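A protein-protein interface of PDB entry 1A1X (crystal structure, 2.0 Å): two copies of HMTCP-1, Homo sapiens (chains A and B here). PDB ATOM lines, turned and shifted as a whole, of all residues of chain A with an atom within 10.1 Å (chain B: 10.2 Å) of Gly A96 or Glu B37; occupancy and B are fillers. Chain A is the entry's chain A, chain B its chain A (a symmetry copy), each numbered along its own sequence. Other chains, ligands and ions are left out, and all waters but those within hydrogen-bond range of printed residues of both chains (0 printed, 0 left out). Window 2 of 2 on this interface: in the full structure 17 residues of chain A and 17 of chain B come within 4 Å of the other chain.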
ATOM      1  N   GLY A   4     -17.204 -32.788  18.688  1.00  0.00           N
ATOM      2  CA  GLY A   4     -16.735 -33.235  19.984  1.00  0.00           C
ATOM      3  C   GLY A   4     -17.082 -32.180  21.009  1.00  0.00           C
ATOM      4  O   GLY A   4     -16.635 -32.252  22.144  1.00  0.00           O
ATOM      5  N   GLU A   5     -17.887 -31.200  20.590  1.00  0.00           N
ATOM      6  CA  GLU A   5     -18.325 -30.092  21.444  1.00  0.00           C
ATOM      7  C   GLU A   5     -19.815 -30.155  21.735  1.00  0.00           C
ATOM      8  O   GLU A   5     -20.564 -30.868  21.067  1.00  0.00           O
ATOM      9  CB  GLU A   5     -18.064 -28.740  20.764  1.00  0.00           C
ATOM     10  CG  GLU A   5     -16.611 -28.331  20.604  1.00  0.00           C
ATOM     11  CD  GLU A   5     -15.948 -27.933  21.909  1.00  0.00           C
ATOM     12  OE1 GLU A   5     -16.454 -27.021  22.587  1.00  0.00           O
ATOM     13  OE2 GLU A   5     -14.901 -28.517  22.241  1.00  0.00           O
ATOM     14  N   VAL A   7     -21.335 -27.020  22.127  1.00  0.00           N
ATOM     15  CA  VAL A   7     -21.483 -25.568  21.966  1.00  0.00           C
ATOM     16  C   VAL A   7     -22.799 -25.174  21.297  1.00  0.00           C
ATOM     17  O   VAL A   7     -23.267 -24.045  21.447  1.00  0.00           O
ATOM     18  CB  VAL A   7     -20.284 -24.966  21.170  1.00  0.00           C
ATOM     19  CG1 VAL A   7     -20.314 -25.435  19.729  1.00  0.00           C
ATOM     20  CG2 VAL A   7     -20.282 -23.453  21.249  1.00  0.00           C
ATOM     21  N   ARG A  28     -27.105 -10.367  21.339  1.00  0.00           N
ATOM     22  CA  ARG A  28     -25.867 -10.611  22.060  1.00  0.00           C
ATOM     23  C   ARG A  28     -24.706 -10.059  21.239  1.00  0.00           C
ATOM     24  O   ARG A  28     -24.718 -10.109  20.008  1.00  0.00           O
ATOM     25  CB  ARG A  28     -25.669 -12.106  22.285  1.00  0.00           C
ATOM     26  CG  ARG A  28     -26.702 -12.725  23.191  1.00  0.00           C
ATOM     27  CD  ARG A  28     -26.432 -14.185  23.353  1.00  0.00           C
ATOM     28  NE  ARG A  28     -26.326 -14.829  22.052  1.00  0.00           N
ATOM     29  CZ  ARG A  28     -26.008 -16.104  21.873  1.00  0.00           C
ATOM     30  NH1 ARG A  28     -25.760 -16.883  22.921  1.00  0.00           N
ATOM     31  NH2 ARG A  28     -25.931 -16.600  20.643  1.00  0.00           N
ATOM     32  N   TRP A  30     -20.755  -9.835  19.890  1.00  0.00           N
ATOM     33  CA  TRP A  30     -19.636 -10.686  19.518  1.00  0.00           C
ATOM     34  C   TRP A  30     -18.505  -9.756  19.132  1.00  0.00           C
ATOM     35  O   TRP A  30     -18.739  -8.752  18.464  1.00  0.00           O
ATOM     36  CB  TRP A  30     -20.003 -11.532  18.312  1.00  0.00           C
ATOM     37  CG  TRP A  30     -20.969 -12.618  18.596  1.00  0.00           C
ATOM     38  CD1 TRP A  30     -22.315 -12.488  18.799  1.00  0.00           C
ATOM     39  CD2 TRP A  30     -20.682 -14.018  18.676  1.00  0.00           C
ATOM     40  NE1 TRP A  30     -22.882 -13.722  18.995  1.00  0.00           N
ATOM     41  CE2 TRP A  30     -21.904 -14.681  18.925  1.00  0.00           C
ATOM     42  CE3 TRP A  30     -19.512 -14.780  18.558  1.00  0.00           C
ATOM     43  CZ2 TRP A  30     -21.991 -16.072  19.056  1.00  0.00           C
ATOM     44  CZ3 TRP A  30     -19.599 -16.167  18.686  1.00  0.00           C
ATOM     45  CH2 TRP A  30     -20.831 -16.795  18.932  1.00  0.00           C
ATOM     46  N   GLN A  46     -15.628 -13.938  19.139  1.00  0.00           N
ATOM     47  CA  GLN A  46     -16.027 -14.439  20.446  1.00  0.00           C
ATOM     48  C   GLN A  46     -17.236 -13.711  21.022  1.00  0.00           C
ATOM     49  O   GLN A  46     -17.335 -12.480  20.952  1.00  0.00           O
ATOM     50  CB  GLN A  46     -14.857 -14.346  21.431  1.00  0.00           C
ATOM     51  CG  GLN A  46     -13.690 -15.250  21.091  1.00  0.00           C
ATOM     52  CD  GLN A  46     -12.607 -15.200  22.140  1.00  0.00           C
ATOM     53  OE1 GLN A  46     -12.651 -14.372  23.040  1.00  0.00           O
ATOM     54  NE2 GLN A  46     -11.623 -16.092  22.032  1.00  0.00           N
ATOM     55  N   GLN A  47     -18.136 -14.487  21.621  1.00  0.00           N
ATOM     56  CA  GLN A  47     -19.346 -13.950  22.228  1.00  0.00           C
ATOM     57  C   GLN A  47     -19.010 -13.428  23.618  1.00  0.00           C
ATOM     58  O   GLN A  47     -18.960 -14.179  24.594  1.00  0.00           O
ATOM     59  CB  GLN A  47     -20.436 -15.029  22.291  1.00  0.00           C
ATOM     60  CG  GLN A  47     -21.863 -14.487  22.290  1.00  0.00           C
ATOM     61  CD  GLN A  47     -22.275 -13.925  23.630  1.00  0.00           C
ATOM     62  OE1 GLN A  47     -22.700 -14.673  24.511  1.00  0.00           O
ATOM     63  NE2 GLN A  47     -22.148 -12.610  23.801  1.00  0.00           N
ATOM     64  N   ILE A  48     -18.724 -12.136  23.672  1.00  0.00           N
ATOM     65  CA  ILE A  48     -18.389 -11.455  24.908  1.00  0.00           C
ATOM     66  C   ILE A  48     -19.271 -10.218  25.017  1.00  0.00           C
ATOM     67  O   ILE A  48     -19.459  -9.486  24.037  1.00  0.00           O
ATOM     68  CB  ILE A  48     -16.897 -11.033  24.920  1.00  0.00           C
ATOM     69  CG1 ILE A  48     -16.003 -12.281  24.825  1.00  0.00           C
ATOM     70  CG2 ILE A  48     -16.571 -10.214  26.185  1.00  0.00           C
ATOM     71  CD1 ILE A  48     -14.507 -11.979  24.703  1.00  0.00           C
ATOM     72  N   GLN A  49     -19.836 -10.019  26.205  1.00  0.00           N
ATOM     73  CA  GLN A  49     -20.694  -8.876  26.508  1.00  0.00           C
ATOM     74  C   GLN A  49     -19.849  -7.599  26.602  1.00  0.00           C
ATOM     75  O   GLN A  49     -18.980  -7.476  27.463  1.00  0.00           O
ATOM     76  CB  GLN A  49     -21.411  -9.135  27.832  1.00  0.00           C
ATOM     77  CG  GLN A  49     -22.408  -8.072  28.255  1.00  0.00           C
ATOM     78  CD  GLN A  49     -23.175  -8.482  29.504  1.00  0.00           C
ATOM     79  OE1 GLN A  49     -23.915  -9.479  29.501  1.00  0.00           O
ATOM     80  NE2 GLN A  49     -22.988  -7.729  30.585  1.00  0.00           N
ATOM     81  N   LEU A  92     -16.168 -23.522  19.024  1.00  0.00           N
ATOM     82  CA  LEU A  92     -15.991 -24.145  20.316  1.00  0.00           C
ATOM     83  C   LEU A  92     -16.014 -23.183  21.483  1.00  0.00           C
ATOM     84  O   LEU A  92     -16.135 -21.968  21.313  1.00  0.00           O
ATOM     85  CB  LEU A  92     -14.698 -24.978  20.330  1.00  0.00           C
ATOM     86  CG  LEU A  92     -13.542 -24.587  19.403  1.00  0.00           C
ATOM     87  CD1 LEU A  92     -12.772 -23.449  19.983  1.00  0.00           C
ATOM     88  CD2 LEU A  92     -12.629 -25.762  19.182  1.00  0.00           C
ATOM     89  N   MET A  93     -15.992 -23.768  22.672  1.00  0.00           N
ATOM     90  CA  MET A  93     -15.985 -23.041  23.925  1.00  0.00           C
ATOM     91  C   MET A  93     -14.522 -22.989  24.346  1.00  0.00           C
ATOM     92  O   MET A  93     -13.874 -24.035  24.479  1.00  0.00           O
ATOM     93  CB  MET A  93     -16.787 -23.827  24.960  1.00  0.00           C
ATOM     94  CG  MET A  93     -17.332 -22.994  26.105  1.00  0.00           C
ATOM     95  SD  MET A  93     -18.586 -21.825  25.530  1.00  0.00           S
ATOM     96  CE  MET A  93     -19.509 -22.829  24.412  1.00  0.00           C
ATOM     97  N   VAL A  94     -13.981 -21.782  24.472  1.00  0.00           N
ATOM     98  CA  VAL A  94     -12.589 -21.611  24.878  1.00  0.00           C
ATOM     99  C   VAL A  94     -12.544 -20.750  26.130  1.00  0.00           C
ATOM    100  O   VAL A  94     -12.935 -19.588  26.109  1.00  0.00           O
ATOM    101  CB  VAL A  94     -11.748 -20.942  23.788  1.00  0.00           C
ATOM    102  CG1 VAL A  94     -10.324 -20.766  24.266  1.00  0.00           C
ATOM    103  CG2 VAL A  94     -11.760 -21.770  22.543  1.00  0.00           C
ATOM    104  N   ARG A  95     -12.063 -21.333  27.221  1.00  0.00           N
ATOM    105  CA  ARG A  95     -11.982 -20.636  28.498  1.00  0.00           C
ATOM    106  C   ARG A  95     -13.348 -20.080  28.914  1.00  0.00           C
ATOM    107  O   ARG A  95     -13.442 -19.017  29.526  1.00  0.00           O
ATOM    108  CB  ARG A  95     -10.909 -19.539  28.452  1.00  0.00           C
ATOM    109  CG  ARG A  95      -9.473 -20.049  28.662  1.00  0.00           C
ATOM    110  CD  ARG A  95      -9.026 -21.044  27.590  1.00  0.00           C
ATOM    111  NE  ARG A  95      -7.694 -21.600  27.851  1.00  0.00           N
ATOM    112  CZ  ARG A  95      -6.702 -21.636  26.960  1.00  0.00           C
ATOM    113  NH1 ARG A  95      -6.875 -21.149  25.734  1.00  0.00           N
ATOM    114  NH2 ARG A  95      -5.526 -22.154  27.298  1.00  0.00           N
ATOM    115  N   GLY A  96     -14.403 -20.811  28.558  1.00  0.00           N
ATOM    116  CA  GLY A  96     -15.758 -20.412  28.910  1.00  0.00           C
ATOM    117  C   GLY A  96     -16.471 -19.478  27.951  1.00  0.00           C
ATOM    118  O   GLY A  96     -17.639 -19.146  28.171  1.00  0.00           O
ATOM    119  N   VAL A  97     -15.787 -19.073  26.884  1.00  0.00           N
ATOM    120  CA  VAL A  97     -16.354 -18.168  25.884  1.00  0.00           C
ATOM    121  C   VAL A  97     -16.553 -18.876  24.553  1.00  0.00           C
ATOM    122  O   VAL A  97     -15.659 -19.583  24.076  1.00  0.00           O
ATOM    123  CB  VAL A  97     -15.427 -16.951  25.665  1.00  0.00           C
ATOM    124  CG1 VAL A  97     -15.969 -16.040  24.579  1.00  0.00           C
ATOM    125  CG2 VAL A  97     -15.278 -16.182  26.954  1.00  0.00           C
ATOM    126  N   GLN A  98     -17.724 -18.681  23.953  1.00  0.00           N
ATOM    127  CA  GLN A  98     -18.041 -19.280  22.659  1.00  0.00           C
ATOM    128  C   GLN A  98     -17.194 -18.583  21.586  1.00  0.00           C
ATOM    129  O   GLN A  98     -17.127 -17.346  21.533  1.00  0.00           O
ATOM    130  CB  GLN A  98     -19.529 -19.129  22.348  1.00  0.00           C
ATOM    131  CG  GLN A  98     -19.999 -19.958  21.175  1.00  0.00           C
ATOM    132  CD  GLN A  98     -21.498 -19.871  20.968  1.00  0.00           C
ATOM    133  OE1 GLN A  98     -22.010 -20.218  19.902  1.00  0.00           O
ATOM    134  NE2 GLN A  98     -22.212 -19.407  21.991  1.00  0.00           N
ATOM    135  N   GLU A  99     -16.562 -19.380  20.730  1.00  0.00           N
ATOM    136  CA  GLU A  99     -15.693 -18.830  19.702  1.00  0.00           C
ATOM    137  C   GLU A  99     -15.883 -19.403  18.300  1.00  0.00           C
ATOM    138  O   GLU A  99     -15.989 -20.613  18.119  1.00  0.00           O
ATOM    139  CB  GLU A  99     -14.230 -19.006  20.127  1.00  0.00           C
ATOM    140  CG  GLU A  99     -13.233 -18.637  19.046  1.00  0.00           C
ATOM    141  CD  GLU A  99     -11.805 -18.876  19.463  1.00  0.00           C
ATOM    142  OE1 GLU A  99     -11.283 -18.108  20.291  1.00  0.00           O
ATOM    143  OE2 GLU A  99     -11.191 -19.820  18.949  1.00  0.00           O
ATOM    144  N   VAL B  33       1.139 -28.468  24.109  1.00  0.00           N
ATOM    145  CA  VAL B  33       0.802 -27.720  25.304  1.00  0.00           C
ATOM    146  C   VAL B  33      -0.616 -28.078  25.735  1.00  0.00           C
ATOM    147  O   VAL B  33      -1.469 -28.392  24.906  1.00  0.00           O
ATOM    148  CB  VAL B  33       0.912 -26.174  25.112  1.00  0.00           C
ATOM    149  CG1 VAL B  33       2.335 -25.777  24.775  1.00  0.00           C
ATOM    150  CG2 VAL B  33      -0.059 -25.677  24.053  1.00  0.00           C
ATOM    151  N   VAL B  34      -0.847 -28.058  27.043  1.00  0.00           N
ATOM    152  CA  VAL B  34      -2.158 -28.366  27.584  1.00  0.00           C
ATOM    153  C   VAL B  34      -2.977 -27.094  27.758  1.00  0.00           C
ATOM    154  O   VAL B  34      -2.468 -26.081  28.218  1.00  0.00           O
ATOM    155  CB  VAL B  34      -2.058 -29.093  28.964  1.00  0.00           C
ATOM    156  CG1 VAL B  34      -3.463 -29.326  29.548  1.00  0.00           C
ATOM    157  CG2 VAL B  34      -1.328 -30.425  28.822  1.00  0.00           C
ATOM    158  N   GLU B  35      -4.228 -27.146  27.318  1.00  0.00           N
ATOM    159  CA  GLU B  35      -5.166 -26.035  27.475  1.00  0.00           C
ATOM    160  C   GLU B  35      -6.417 -26.666  28.074  1.00  0.00           C
ATOM    161  O   GLU B  35      -7.306 -27.142  27.374  1.00  0.00           O
ATOM    162  CB  GLU B  35      -5.439 -25.378  26.137  1.00  0.00           C
ATOM    163  CG  GLU B  35      -4.155 -24.923  25.497  1.00  0.00           C
ATOM    164  CD  GLU B  35      -4.367 -24.039  24.300  1.00  0.00           C
ATOM    165  OE1 GLU B  35      -5.315 -24.310  23.529  1.00  0.00           O
ATOM    166  OE2 GLU B  35      -3.576 -23.078  24.132  1.00  0.00           O
ATOM    167  N   GLU B  36      -6.429 -26.723  29.395  1.00  0.00           N
ATOM    168  CA  GLU B  36      -7.507 -27.345  30.137  1.00  0.00           C
ATOM    169  C   GLU B  36      -8.752 -26.498  30.379  1.00  0.00           C
ATOM    170  O   GLU B  36      -8.673 -25.372  30.871  1.00  0.00           O
ATOM    171  CB  GLU B  36      -6.949 -27.835  31.460  1.00  0.00           C
ATOM    172  CG  GLU B  36      -7.864 -28.744  32.222  1.00  0.00           C
ATOM    173  CD  GLU B  36      -7.253 -29.197  33.524  1.00  0.00           C
ATOM    174  OE1 GLU B  36      -6.005 -29.256  33.619  1.00  0.00           O
ATOM    175  OE2 GLU B  36      -8.027 -29.486  34.458  1.00  0.00           O
ATOM    176  N   GLU B  37      -9.903 -27.043  29.993  1.00  0.00           N
ATOM    177  CA  GLU B  37     -11.185 -26.377  30.200  1.00  0.00           C
ATOM    178  C   GLU B  37     -11.736 -26.903  31.526  1.00  0.00           C
ATOM    179  O   GLU B  37     -11.070 -27.690  32.210  1.00  0.00           O
ATOM    180  CB  GLU B  37     -12.148 -26.709  29.055  1.00  0.00           C
ATOM    181  CG  GLU B  37     -11.639 -26.325  27.666  1.00  0.00           C
ATOM    182  CD  GLU B  37     -11.388 -24.838  27.512  1.00  0.00           C
ATOM    183  OE1 GLU B  37     -12.205 -24.045  28.023  1.00  0.00           O
ATOM    184  OE2 GLU B  37     -10.376 -24.464  26.876  1.00  0.00           O
ATOM    185  N   THR B  38     -12.942 -26.481  31.896  1.00  0.00           N
ATOM    186  CA  THR B  38     -13.544 -26.938  33.151  1.00  0.00           C
ATOM    187  C   THR B  38     -13.962 -28.414  33.093  1.00  0.00           C
ATOM    188  O   THR B  38     -13.664 -29.208  33.993  1.00  0.00           O
ATOM    189  CB  THR B  38     -14.793 -26.093  33.526  1.00  0.00           C
ATOM    190  OG1 THR B  38     -14.407 -24.735  33.753  1.00  0.00           O
ATOM    191  CG2 THR B  38     -15.444 -26.632  34.791  1.00  0.00           C
ATOM    192  N   SER B  39     -14.621 -28.773  32.004  1.00  0.00           N
ATOM    193  CA  SER B  39     -15.128 -30.110  31.823  1.00  0.00           C
ATOM    194  C   SER B  39     -14.252 -31.051  31.021  1.00  0.00           C
ATOM    195  O   SER B  39     -14.510 -32.252  30.995  1.00  0.00           O
ATOM    196  CB  SER B  39     -16.502 -30.021  31.186  1.00  0.00           C
ATOM    197  OG  SER B  39     -17.257 -29.034  31.863  1.00  0.00           O
ATOM    198  N   PHE B  40     -13.228 -30.527  30.355  1.00  0.00           N
ATOM    199  CA  PHE B  40     -12.359 -31.391  29.554  1.00  0.00           C
ATOM    200  C   PHE B  40     -10.977 -30.815  29.310  1.00  0.00           C
ATOM    201  O   PHE B  40     -10.664 -29.694  29.717  1.00  0.00           O
ATOM    202  CB  PHE B  40     -13.021 -31.753  28.212  1.00  0.00           C
ATOM    203  CG  PHE B  40     -13.442 -30.566  27.423  1.00  0.00           C
ATOM    204  CD1 PHE B  40     -14.694 -30.000  27.623  1.00  0.00           C
ATOM    205  CD2 PHE B  40     -12.568 -29.965  26.532  1.00  0.00           C
ATOM    206  CE1 PHE B  40     -15.069 -28.837  26.945  1.00  0.00           C
ATOM    207  CE2 PHE B  40     -12.932 -28.805  25.850  1.00  0.00           C
ATOM    208  CZ  PHE B  40     -14.186 -28.239  26.059  1.00  0.00           C
ATOM    209  N   LEU B  41     -10.170 -31.594  28.602  1.00  0.00           N
ATOM    210  CA  LEU B  41      -8.812 -31.212  28.299  1.00  0.00           C
ATOM    211  C   LEU B  41      -8.526 -31.204  26.807  1.00  0.00           C
ATOM    212  O   LEU B  41      -8.996 -32.065  26.060  1.00  0.00           O
ATOM    213  CB  LEU B  41      -7.867 -32.168  29.021  1.00  0.00           C
ATOM    214  CG  LEU B  41      -6.377 -31.878  28.947  1.00  0.00           C
ATOM    215  CD1 LEU B  41      -5.766 -32.045  30.326  1.00  0.00           C
ATOM    216  CD2 LEU B  41      -5.725 -32.786  27.930  1.00  0.00           C
ATOM    217  N   ARG B  42      -7.784 -30.191  26.382  1.00  0.00           N
ATOM    218  CA  ARG B  42      -7.373 -30.035  24.993  1.00  0.00           C
ATOM    219  C   ARG B  42      -5.851 -29.935  24.948  1.00  0.00           C
ATOM    220  O   ARG B  42      -5.217 -29.516  25.914  1.00  0.00           O
ATOM    221  CB  ARG B  42      -7.958 -28.756  24.368  1.00  0.00           C
ATOM    222  CG  ARG B  42      -9.449 -28.814  24.025  1.00  0.00           C
ATOM    223  CD  ARG B  42      -9.796 -27.801  22.917  1.00  0.00           C
ATOM    224  NE  ARG B  42     -11.240 -27.617  22.757  1.00  0.00           N
ATOM    225  CZ  ARG B  42     -11.942 -26.616  23.286  1.00  0.00           C
ATOM    226  NH1 ARG B  42     -11.346 -25.685  24.017  1.00  0.00           N
ATOM    227  NH2 ARG B  42     -13.252 -26.554  23.100  1.00  0.00           N
ATOM    228  N   ALA B  43      -5.269 -30.370  23.840  1.00  0.00           N
ATOM    229  CA  ALA B  43      -3.830 -30.279  23.646  1.00  0.00           C
ATOM    230  C   ALA B  43      -3.644 -29.565  22.317  1.00  0.00           C
ATOM    231  O   ALA B  43      -4.289 -29.905  21.340  1.00  0.00           O
ATOM    232  CB  ALA B  43      -3.203 -31.661  23.593  1.00  0.00           C
ATOM    233  N   ARG B  44      -2.837 -28.516  22.312  1.00  0.00           N
ATOM    234  CA  ARG B  44      -2.563 -27.776  21.091  1.00  0.00           C
ATOM    235  C   ARG B  44      -1.156 -28.218  20.715  1.00  0.00           C
ATOM    236  O   ARG B  44      -0.223 -28.078  21.498  1.00  0.00           O
ATOM    237  CB  ARG B  44      -2.638 -26.272  21.348  1.00  0.00           C
ATOM    238  CG  ARG B  44      -2.574 -25.426  20.088  1.00  0.00           C
ATOM    239  CD  ARG B  44      -3.303 -24.110  20.297  1.00  0.00           C
ATOM    240  NE  ARG B  44      -2.765 -23.372  21.428  1.00  0.00           N
ATOM    241  CZ  ARG B  44      -1.711 -22.565  21.370  1.00  0.00           C
ATOM    242  NH1 ARG B  44      -1.064 -22.381  20.226  1.00  0.00           N
ATOM    243  NH2 ARG B  44      -1.313 -21.931  22.461  1.00  0.00           N
ATOM    244  N   GLN B  65      -0.053 -35.236  31.842  1.00  0.00           N
ATOM    245  CA  GLN B  65      -1.440 -35.176  31.362  1.00  0.00           C
ATOM    246  C   GLN B  65      -1.526 -35.638  29.894  1.00  0.00           C
ATOM    247  O   GLN B  65      -2.587 -36.043  29.411  1.00  0.00           O
ATOM    248  CB  GLN B  65      -1.993 -33.752  31.494  1.00  0.00           C
ATOM    249  CG  GLN B  65      -2.131 -33.274  32.933  1.00  0.00           C
ATOM    250  CD  GLN B  65      -2.721 -31.883  33.017  1.00  0.00           C
ATOM    251  OE1 GLN B  65      -2.021 -30.894  32.829  1.00  0.00           O
ATOM    252  NE2 GLN B  65      -4.017 -31.801  33.279  1.00  0.00           N
ATOM    253  N   GLN B  89     -10.006 -31.352  16.536  1.00  0.00           N
ATOM    254  CA  GLN B  89     -10.979 -30.269  16.370  1.00  0.00           C
ATOM    255  C   GLN B  89     -10.601 -29.350  15.221  1.00  0.00           C
ATOM    256  O   GLN B  89     -11.467 -28.759  14.570  1.00  0.00           O
ATOM    257  CB  GLN B  89     -11.176 -29.514  17.673  1.00  0.00           C
ATOM    258  CG  GLN B  89     -11.640 -30.432  18.778  1.00  0.00           C
ATOM    259  CD  GLN B  89     -12.264 -29.672  19.910  1.00  0.00           C
ATOM    260  OE1 GLN B  89     -11.571 -29.094  20.735  1.00  0.00           O
ATOM    261  NE2 GLN B  89     -13.587 -29.660  19.953  1.00  0.00           N
ATOM    262  N   LEU B 101      -5.323 -29.280  16.982  1.00  0.00           N
ATOM    263  CA  LEU B 101      -6.042 -28.968  18.211  1.00  0.00           C
ATOM    264  C   LEU B 101      -6.802 -30.245  18.552  1.00  0.00           C
ATOM    265  O   LEU B 101      -7.766 -30.613  17.867  1.00  0.00           O
ATOM    266  CB  LEU B 101      -7.006 -27.785  18.052  1.00  0.00           C
ATOM    267  CG  LEU B 101      -7.662 -27.438  19.399  1.00  0.00           C
ATOM    268  CD1 LEU B 101      -6.602 -26.948  20.375  1.00  0.00           C
ATOM    269  CD2 LEU B 101      -8.772 -26.405  19.222  1.00  0.00           C
ATOM    270  N   LEU B 102      -6.321 -30.931  19.590  1.00  0.00           N
ATOM    271  CA  LEU B 102      -6.882 -32.202  20.053  1.00  0.00           C
ATOM    272  C   LEU B 102      -7.723 -32.079  21.313  1.00  0.00           C
ATOM    273  O   LEU B 102      -7.367 -31.361  22.241  1.00  0.00           O
ATOM    274  CB  LEU B 102      -5.748 -33.195  20.331  1.00  0.00           C
ATOM    275  CG  LEU B 102      -4.760 -33.463  19.201  1.00  0.00           C
ATOM    276  CD1 LEU B 102      -3.680 -34.447  19.658  1.00  0.00           C
ATOM    277  CD2 LEU B 102      -5.517 -34.002  18.004  1.00  0.00           C
ATOM    278  N   LYS B 103      -8.802 -32.846  21.367  1.00  0.00           N
ATOM    279  CA  LYS B 103      -9.678 -32.828  22.521  1.00  0.00           C
ATOM    280  C   LYS B 103      -9.855 -34.241  23.052  1.00  0.00           C
ATOM    281  O   LYS B 103     -10.311 -35.127  22.329  1.00  0.00           O
ATOM    282  CB  LYS B 103     -11.042 -32.242  22.141  1.00  0.00           C
ATOM    283  CG  LYS B 103     -12.004 -32.085  23.324  1.00  0.00           C
ATOM    284  CD  LYS B 103     -13.330 -31.512  22.887  1.00  0.00           C
ATOM    285  CE  LYS B 103     -14.249 -31.366  24.067  1.00  0.00           C
ATOM    286  NZ  LYS B 103     -15.516 -30.687  23.706  1.00  0.00           N
ATOM    287  N   LEU B 104      -9.490 -34.448  24.313  1.00  0.00           N
ATOM    288  CA  LEU B 104      -9.626 -35.764  24.936  1.00  0.00           C
ATOM    289  C   LEU B 104     -11.095 -36.056  25.196  1.00  0.00           C
ATOM    290  O   LEU B 104     -11.760 -35.323  25.922  1.00  0.00           O
ATOM    291  CB  LEU B 104      -8.838 -35.830  26.246  1.00  0.00           C
ATOM    292  CG  LEU B 104      -8.983 -37.141  27.009  1.00  0.00           C
ATOM    293  CD1 LEU B 104      -8.556 -38.318  26.141  1.00  0.00           C
ATOM    294  CD2 LEU B 104      -8.170 -37.073  28.278  1.00  0.00           C
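The backbone carbonyl oxygen of Gly A4 sits at hydrogen-bond distance from the side-chain amino group of Lys B103. The side-chain carboxylate (OE2) of Glu A5 is in salt-bridge range of the guanidinium group (NH2) of Arg B42, at 2.7 Å. The side-chain carboxylate (OE2) of Glu A5 is in hydrogen-bond range of the side-chain amide nitrogen (NE2) of Gln B89 (2.9 Å). The side-chain carboxylate of Glu A5 is in salt-bridge range of the side-chain amino group of Lys B103, 2.7 Å away. NH2 of Arg B42 is in hydrogen-bond range of O of Met A93. The guanidinium group (NH2) of Arg A95 lies within salt-bridge range of the side-chain carboxylate (OE2) of Glu B35, 3.8 Å away. N of Arg A95 lies within hydrogen-bond range of OE1 of Glu B37, at 2.8 Å.
N of Met A93 sits at hydrogen-bond distance from OE1 of Glu A5 (3.3 Å). The side-chain sulfur (SD) of Met A93 lies within hydrogen-bond range of the backbone NH (N) of Gln A98 (3.6 Å). N of Glu B35 is in hydrogen-bond range of O of Arg B42 (2.9 Å). The guanidinium group of Arg B44 is in salt-bridge range of the side-chain carboxylate of Glu B35 (2.8 Å). OE1 of Gln B89 is in hydrogen-bond range of NE of Arg B42. N of Gln B89 sits at hydrogen-bond distance from O of Leu B101 (2.7 Å).
Among the printed residues, pairs that only touch across the chains: Glu A5 with Phe B40 (3.9 Å), Leu A92 with Arg B42 (3.5 Å), Leu A92 with Gln B89 (3.8 Å), Leu A92 with Leu B101 (3.9 Å), Met A93 with Glu B37 (3.9 Å), Val A94 with Glu B37 (3.8 Å) and Gly A96 with Glu B37 (3.9 Å).
Printed residues of chain B within 4 Å of Gly A4: Lys B103. Of chain B, only Glu B35 (3.4 Å) and Glu B37 (2.8 Å) come within 4 Å of Arg A95. Gly A96 touches just one residue of chain B: Glu B37. No residue of chain B comes within 4 Å of Val A97. No residue of chain A comes within 4 Å of Glu B36. Of the printed residues of chain A, Glu B37 touches Met A93, Val A94, Arg A95 and Gly A96. No residue of chain A comes within 4 Å of Thr B38. No residue of chain A comes within 4 Å of Ser B39. Phe B40 touches one residue of chain A. Printed residues of chain A within 4 Å of Arg B42: Glu A5, Leu A92 and Met A93. Printed residues of chain A within 4 Å of Lys B103: Gly A4 (2.5 Å) and Glu A5 (2.7 Å). The nearest residue of chain B that does not touch Gly A96 is Thr B38 (6.5 Å). The nearest residue of chain A that does not touch Glu B37 is Val A97 (6.2 Å).
Hydrophobic or aromatic side chains of chain A within 4 Å of the printed part of chain B: Leu A92. Of the 18 printed residues of chain B, 7 touch a printed residue of chain A. Among the printed residues, 14 pairs touch across the chains.
No position is printed for both chains. Of the 14 pairs that touch across the chains among the printed residues, none has its exchanged pair printed and touching as well.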
